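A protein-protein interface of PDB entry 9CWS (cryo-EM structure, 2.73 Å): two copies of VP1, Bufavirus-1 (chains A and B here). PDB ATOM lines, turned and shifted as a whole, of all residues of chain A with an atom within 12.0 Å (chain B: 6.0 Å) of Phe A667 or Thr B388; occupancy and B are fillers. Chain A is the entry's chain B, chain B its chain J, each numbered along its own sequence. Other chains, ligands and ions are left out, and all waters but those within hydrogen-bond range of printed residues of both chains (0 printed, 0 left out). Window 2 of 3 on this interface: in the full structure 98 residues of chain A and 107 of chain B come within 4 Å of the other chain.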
ATOM      1  N   LEU A 663      -3.732  14.754  24.405  1.00  0.00           N
ATOM      2  CA  LEU A 663      -4.509  13.603  23.999  1.00  0.00           C
ATOM      3  C   LEU A 663      -5.957  14.011  23.743  1.00  0.00           C
ATOM      4  O   LEU A 663      -6.414  15.028  24.273  1.00  0.00           O
ATOM      5  CB  LEU A 663      -4.451  12.510  25.072  1.00  0.00           C
ATOM      6  CG  LEU A 663      -3.058  11.906  25.271  1.00  0.00           C
ATOM      7  CD1 LEU A 663      -3.057  10.927  26.420  1.00  0.00           C
ATOM      8  CD2 LEU A 663      -2.578  11.233  24.000  1.00  0.00           C
ATOM      9  N   PRO A 664      -6.702  13.262  22.917  1.00  0.00           N
ATOM     10  CA  PRO A 664      -8.059  13.700  22.560  1.00  0.00           C
ATOM     11  C   PRO A 664      -8.989  13.805  23.758  1.00  0.00           C
ATOM     12  O   PRO A 664      -9.130  12.858  24.534  1.00  0.00           O
ATOM     13  CB  PRO A 664      -8.530  12.610  21.588  1.00  0.00           C
ATOM     14  CG  PRO A 664      -7.289  12.032  21.044  1.00  0.00           C
ATOM     15  CD  PRO A 664      -6.302  12.064  22.161  1.00  0.00           C
ATOM     16  N   ARG A 665      -9.616  14.966  23.921  1.00  0.00           N
ATOM     17  CA  ARG A 665     -10.604  15.194  24.965  1.00  0.00           C
ATOM     18  C   ARG A 665     -12.033  15.106  24.444  1.00  0.00           C
ATOM     19  O   ARG A 665     -12.981  15.365  25.183  1.00  0.00           O
ATOM     20  CB  ARG A 665     -10.379  16.537  25.652  1.00  0.00           C
ATOM     21  CG  ARG A 665      -9.056  16.641  26.380  1.00  0.00           C
ATOM     22  CD  ARG A 665      -9.003  17.901  27.205  1.00  0.00           C
ATOM     23  NE  ARG A 665      -9.974  17.839  28.294  1.00  0.00           N
ATOM     24  CZ  ARG A 665     -10.246  18.844  29.117  1.00  0.00           C
ATOM     25  NH1 ARG A 665     -11.142  18.691  30.077  1.00  0.00           N
ATOM     26  NH2 ARG A 665      -9.629  20.006  28.975  1.00  0.00           N
ATOM     27  N   GLN A 666     -12.207  14.771  23.173  1.00  0.00           N
ATOM     28  CA  GLN A 666     -13.525  14.827  22.568  1.00  0.00           C
ATOM     29  C   GLN A 666     -13.721  13.601  21.696  1.00  0.00           C
ATOM     30  O   GLN A 666     -12.764  12.921  21.326  1.00  0.00           O
ATOM     31  CB  GLN A 666     -13.692  16.103  21.750  1.00  0.00           C
ATOM     32  CG  GLN A 666     -12.788  16.141  20.559  1.00  0.00           C
ATOM     33  CD  GLN A 666     -12.903  17.412  19.789  1.00  0.00           C
ATOM     34  OE1 GLN A 666     -13.261  18.440  20.331  1.00  0.00           O
ATOM     35  NE2 GLN A 666     -12.636  17.346  18.500  1.00  0.00           N
ATOM     36  N   PHE A 667     -14.985  13.320  21.392  1.00  0.00           N
ATOM     37  CA  PHE A 667     -15.366  12.246  20.490  1.00  0.00           C
ATOM     38  C   PHE A 667     -15.184  12.637  19.035  1.00  0.00           C
ATOM     39  O   PHE A 667     -14.640  11.860  18.251  1.00  0.00           O
ATOM     40  CB  PHE A 667     -16.828  11.868  20.738  1.00  0.00           C
ATOM     41  CG  PHE A 667     -17.315  10.690  19.943  1.00  0.00           C
ATOM     42  CD1 PHE A 667     -17.191   9.413  20.438  1.00  0.00           C
ATOM     43  CD2 PHE A 667     -17.906  10.862  18.709  1.00  0.00           C
ATOM     44  CE1 PHE A 667     -17.646   8.340  19.721  1.00  0.00           C
ATOM     45  CE2 PHE A 667     -18.350   9.789  17.991  1.00  0.00           C
ATOM     46  CZ  PHE A 667     -18.220   8.528  18.498  1.00  0.00           C
ATOM     47  N   ASN A 668     -15.629  13.834  18.669  1.00  0.00           N
ATOM     48  CA  ASN A 668     -15.573  14.287  17.294  1.00  0.00           C
ATOM     49  C   ASN A 668     -14.151  14.651  16.884  1.00  0.00           C
ATOM     50  O   ASN A 668     -13.261  14.867  17.704  1.00  0.00           O
ATOM     51  CB  ASN A 668     -16.497  15.482  17.076  1.00  0.00           C
ATOM     52  CG  ASN A 668     -16.199  16.620  18.006  1.00  0.00           C
ATOM     53  OD1 ASN A 668     -15.658  16.421  19.078  1.00  0.00           O
ATOM     54  ND2 ASN A 668     -16.504  17.828  17.579  1.00  0.00           N
ATOM     55  N   LEU A 669     -13.970  14.673  15.560  1.00  0.00           N
ATOM     56  CA  LEU A 669     -12.627  14.937  14.988  1.00  0.00           C
ATOM     57  C   LEU A 669     -12.300  16.425  15.048  1.00  0.00           C
ATOM     58  O   LEU A 669     -13.191  17.245  14.752  1.00  0.00           O
ATOM     59  CB  LEU A 669     -12.613  14.426  13.542  1.00  0.00           C
ATOM     60  CG  LEU A 669     -11.328  14.672  12.753  1.00  0.00           C
ATOM     61  CD1 LEU A 669     -10.158  13.935  13.388  1.00  0.00           C
ATOM     62  CD2 LEU A 669     -11.492  14.246  11.304  1.00  0.00           C
ATOM     63  N   TYR A 670     -11.065  16.745  15.411  1.00  0.00           N
ATOM     64  CA  TYR A 670     -10.581  18.121  15.488  1.00  0.00           C
ATOM     65  C   TYR A 670     -10.475  18.717  14.093  1.00  0.00           C
ATOM     66  O   TYR A 670      -9.811  18.153  13.219  1.00  0.00           O
ATOM     67  CB  TYR A 670      -9.222  18.190  16.179  1.00  0.00           C
ATOM     68  CG  TYR A 670      -9.250  17.934  17.662  1.00  0.00           C
ATOM     69  CD1 TYR A 670      -9.394  18.978  18.560  1.00  0.00           C
ATOM     70  CD2 TYR A 670      -9.147  16.647  18.165  1.00  0.00           C
ATOM     71  CE1 TYR A 670      -9.423  18.751  19.915  1.00  0.00           C
ATOM     72  CE2 TYR A 670      -9.182  16.408  19.519  1.00  0.00           C
ATOM     73  CZ  TYR A 670      -9.318  17.462  20.390  1.00  0.00           C
ATOM     74  OH  TYR A 670      -9.351  17.219  21.740  1.00  0.00           O
ATOM     75  N   ASN A 671     -11.115  19.863  13.892  1.00  0.00           N
ATOM     76  CA  ASN A 671     -11.045  20.561  12.620  1.00  0.00           C
ATOM     77  C   ASN A 671      -9.982  21.653  12.692  1.00  0.00           C
ATOM     78  O   ASN A 671      -9.352  21.878  13.727  1.00  0.00           O
ATOM     79  CB  ASN A 671     -12.408  21.138  12.263  1.00  0.00           C
ATOM     80  CG  ASN A 671     -13.417  20.070  11.935  1.00  0.00           C
ATOM     81  OD1 ASN A 671     -13.060  18.960  11.555  1.00  0.00           O
ATOM     82  ND2 ASN A 671     -14.692  20.399  12.078  1.00  0.00           N
ATOM     83  N   PRO A 703      -8.916  23.943  20.197  1.00  0.00           N
ATOM     84  CA  PRO A 703      -9.803  24.440  21.252  1.00  0.00           C
ATOM     85  C   PRO A 703      -9.667  23.627  22.526  1.00  0.00           C
ATOM     86  O   PRO A 703      -9.240  22.471  22.506  1.00  0.00           O
ATOM     87  CB  PRO A 703     -11.194  24.288  20.639  1.00  0.00           C
ATOM     88  CG  PRO A 703     -11.046  23.190  19.682  1.00  0.00           C
ATOM     89  CD  PRO A 703      -9.674  23.312  19.107  1.00  0.00           C
ATOM     90  N   ASN A 704     -10.043  24.239  23.641  1.00  0.00           N
ATOM     91  CA  ASN A 704     -10.026  23.544  24.916  1.00  0.00           C
ATOM     92  C   ASN A 704     -11.005  24.227  25.854  1.00  0.00           C
ATOM     93  O   ASN A 704     -11.389  25.378  25.649  1.00  0.00           O
ATOM     94  CB  ASN A 704      -8.617  23.515  25.509  1.00  0.00           C
ATOM     95  CG  ASN A 704      -8.457  22.473  26.584  1.00  0.00           C
ATOM     96  OD1 ASN A 704      -9.115  21.437  26.562  1.00  0.00           O
ATOM     97  ND2 ASN A 704      -7.572  22.735  27.531  1.00  0.00           N
ATOM     98  N   TYR A 705     -11.416  23.502  26.887  1.00  0.00           N
ATOM     99  CA  TYR A 705     -12.345  24.036  27.869  1.00  0.00           C
ATOM    100  C   TYR A 705     -11.620  24.921  28.868  1.00  0.00           C
ATOM    101  O   TYR A 705     -10.521  24.597  29.321  1.00  0.00           O
ATOM    102  CB  TYR A 705     -13.063  22.917  28.617  1.00  0.00           C
ATOM    103  CG  TYR A 705     -13.960  22.062  27.767  1.00  0.00           C
ATOM    104  CD1 TYR A 705     -15.240  22.474  27.447  1.00  0.00           C
ATOM    105  CD2 TYR A 705     -13.542  20.821  27.319  1.00  0.00           C
ATOM    106  CE1 TYR A 705     -16.063  21.693  26.678  1.00  0.00           C
ATOM    107  CE2 TYR A 705     -14.362  20.030  26.558  1.00  0.00           C
ATOM    108  CZ  TYR A 705     -15.620  20.470  26.239  1.00  0.00           C
ATOM    109  OH  TYR A 705     -16.435  19.675  25.478  1.00  0.00           O
ATOM    110  N   PHE B 383     -17.483  17.837  21.437  1.00  0.00           N
ATOM    111  CA  PHE B 383     -18.459  16.893  21.959  1.00  0.00           C
ATOM    112  C   PHE B 383     -17.723  15.775  22.674  1.00  0.00           C
ATOM    113  O   PHE B 383     -17.049  14.961  22.043  1.00  0.00           O
ATOM    114  CB  PHE B 383     -19.346  16.358  20.839  1.00  0.00           C
ATOM    115  CG  PHE B 383     -20.121  15.144  21.219  1.00  0.00           C
ATOM    116  CD1 PHE B 383     -21.116  15.212  22.168  1.00  0.00           C
ATOM    117  CD2 PHE B 383     -19.887  13.942  20.588  1.00  0.00           C
ATOM    118  CE1 PHE B 383     -21.824  14.100  22.510  1.00  0.00           C
ATOM    119  CE2 PHE B 383     -20.607  12.833  20.925  1.00  0.00           C
ATOM    120  CZ  PHE B 383     -21.575  12.914  21.887  1.00  0.00           C
ATOM    121  N   THR B 384     -17.842  15.749  23.995  1.00  0.00           N
ATOM    122  CA  THR B 384     -17.231  14.713  24.816  1.00  0.00           C
ATOM    123  C   THR B 384     -18.297  13.909  25.551  1.00  0.00           C
ATOM    124  O   THR B 384     -18.997  14.451  26.416  1.00  0.00           O
ATOM    125  CB  THR B 384     -16.224  15.335  25.794  1.00  0.00           C
ATOM    126  OG1 THR B 384     -15.696  14.335  26.672  1.00  0.00           O
ATOM    127  CG2 THR B 384     -16.810  16.475  26.578  1.00  0.00           C
ATOM    128  N   PRO B 385     -18.492  12.637  25.221  1.00  0.00           N
ATOM    129  CA  PRO B 385     -19.462  11.822  25.949  1.00  0.00           C
ATOM    130  C   PRO B 385     -18.890  11.340  27.273  1.00  0.00           C
ATOM    131  O   PRO B 385     -17.721  11.530  27.592  1.00  0.00           O
ATOM    132  CB  PRO B 385     -19.697  10.642  25.003  1.00  0.00           C
ATOM    133  CG  PRO B 385     -19.268  11.111  23.696  1.00  0.00           C
ATOM    134  CD  PRO B 385     -18.104  11.995  23.960  1.00  0.00           C
ATOM    135  N   ILE B 386     -19.745  10.678  28.037  1.00  0.00           N
ATOM    136  CA  ILE B 386     -19.320  10.073  29.290  1.00  0.00           C
ATOM    137  C   ILE B 386     -18.647   8.731  29.038  1.00  0.00           C
ATOM    138  O   ILE B 386     -17.747   8.340  29.781  1.00  0.00           O
ATOM    139  CB  ILE B 386     -20.523   9.914  30.237  1.00  0.00           C
ATOM    140  CG1 ILE B 386     -21.345  11.202  30.305  1.00  0.00           C
ATOM    141  CG2 ILE B 386     -20.075   9.498  31.608  1.00  0.00           C
ATOM    142  CD1 ILE B 386     -20.619  12.385  30.731  1.00  0.00           C
ATOM    143  N   GLU B 387     -19.062   8.029  27.983  1.00  0.00           N
ATOM    144  CA  GLU B 387     -18.637   6.654  27.759  1.00  0.00           C
ATOM    145  C   GLU B 387     -17.191   6.560  27.310  1.00  0.00           C
ATOM    146  O   GLU B 387     -16.476   5.648  27.734  1.00  0.00           O
ATOM    147  CB  GLU B 387     -19.552   5.996  26.735  1.00  0.00           C
ATOM    148  CG  GLU B 387     -20.942   5.681  27.248  1.00  0.00           C
ATOM    149  CD  GLU B 387     -21.872   6.865  27.252  1.00  0.00           C
ATOM    150  OE1 GLU B 387     -21.429   7.979  26.932  1.00  0.00           O
ATOM    151  OE2 GLU B 387     -23.061   6.681  27.572  1.00  0.00           O
ATOM    152  N   THR B 388     -16.743   7.474  26.461  1.00  0.00           N
ATOM    153  CA  THR B 388     -15.381   7.461  25.954  1.00  0.00           C
ATOM    154  C   THR B 388     -14.409   8.187  26.868  1.00  0.00           C
ATOM    155  O   THR B 388     -13.222   8.266  26.548  1.00  0.00           O
ATOM    156  CB  THR B 388     -15.336   8.078  24.557  1.00  0.00           C
ATOM    157  OG1 THR B 388     -15.778   9.437  24.617  1.00  0.00           O
ATOM    158  CG2 THR B 388     -16.236   7.310  23.613  1.00  0.00           C
ATOM    159  N   THR B 389     -14.881   8.709  27.993  1.00  0.00           N
ATOM    160  CA  THR B 389     -14.106   9.564  28.879  1.00  0.00           C
ATOM    161  C   THR B 389     -13.741   8.884  30.188  1.00  0.00           C
ATOM    162  O   THR B 389     -12.560   8.793  30.524  1.00  0.00           O
ATOM    163  CB  THR B 389     -14.870  10.864  29.157  1.00  0.00           C
ATOM    164  OG1 THR B 389     -15.130  11.534  27.922  1.00  0.00           O
ATOM    165  CG2 THR B 389     -14.047  11.775  30.028  1.00  0.00           C
ATOM    166  N   THR B 390     -14.725   8.444  30.962  1.00  0.00           N
ATOM    167  CA  THR B 390     -14.487   7.876  32.278  1.00  0.00           C
ATOM    168  C   THR B 390     -14.929   6.419  32.326  1.00  0.00           C
ATOM    169  O   THR B 390     -15.703   5.954  31.489  1.00  0.00           O
ATOM    170  CB  THR B 390     -15.210   8.678  33.377  1.00  0.00           C
ATOM    171  OG1 THR B 390     -16.611   8.726  33.108  1.00  0.00           O
ATOM    172  CG2 THR B 390     -14.681  10.090  33.438  1.00  0.00           C
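The backbone carbonyl oxygen (O) of Arg A665 sits at hydrogen-bond distance from the side-chain hydroxyl (OG1) of Thr B384, at 3.3 Å.
The backbone NH (N) of Phe A667 is in hydrogen-bond range of the backbone carbonyl oxygen (O) of Phe B383, at 2.7 Å.
OD1 of Asn A668 is in hydrogen-bond range of N of Phe B383, at 3.3 Å.
The backbone NH (N) of Arg A665 sits at hydrogen-bond distance from the side-chain hydroxyl (OH) of Tyr A670.
OD1 of Asn A704 is in hydrogen-bond range of NH2 of Arg A665 (2.9 Å).
NE2 of Gln A666 is in hydrogen-bond range of O of Asn A668, at 2.7 Å.
The side-chain hydroxyl of Thr B384 sits at hydrogen-bond distance from the side-chain hydroxyl of Thr B389, at 3.1 Å.
The side-chain hydroxyl (OG1) of Thr B389 sits at hydrogen-bond distance from the backbone carbonyl oxygen (O) of Pro B385, at 2.6 Å.
Among the printed residues, pairs that only touch across the chains: Gln A666 with Phe B383, Phe A667 with Pro B385, Phe A667 with Thr B388 and Tyr A705 with Thr B384.
Printed residues of chain A within 4 Å of Thr B388: Phe A667.
Phe B383 touches just these residues of chain A: Gln A666 (3.6 Å), Phe A667 (2.7 Å) and Asn A668 (3.3 Å).
Thr B384 touches just these residues of chain A: Arg A665 (3.3 Å) and Tyr A705 (3.4 Å).
Of chain A, only Phe A667 (3.5 Å) comes within 4 Å of Pro B385.
No residue of chain A comes within 4 Å of Ile B386.
No residue of chain A comes within 4 Å of Glu B387.
No residue of chain A comes within 4 Å of Thr B389.
No residue of chain A comes within 4 Å of Thr B390.
Of the printed residues of chain B, Gln A666 touches Phe B383.
Printed residues of chain B within 4 Å of Asn A668: Phe B383 (3.3 Å).
Leu A663 touches none of the printed residues of chain B.
Hydrophobic or aromatic side chains of chain B within 4 Å of the printed part of chain A: Phe B383 and Pro B385.
Of the 12 printed residues of chain A, 5 touch a printed residue of chain B.
Hydrophobic or aromatic side chains of chain A within 4 Å of the printed part of chain B: Phe A667 and Tyr A705.
Along chain A the printed residues that touch a printed residue of chain B span positions 665 to 705.
Among the printed residues, 7 pairs touch across the chains.
Among the printed residues, no Asp or Glu carboxylate lies within 4 Å of a Lys or Arg side-chain nitrogen of the other chain.
No position is printed for both chains.
Of the 7 pairs that touch across the chains among the printed residues, none has its exchanged pair printed and touching as well.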
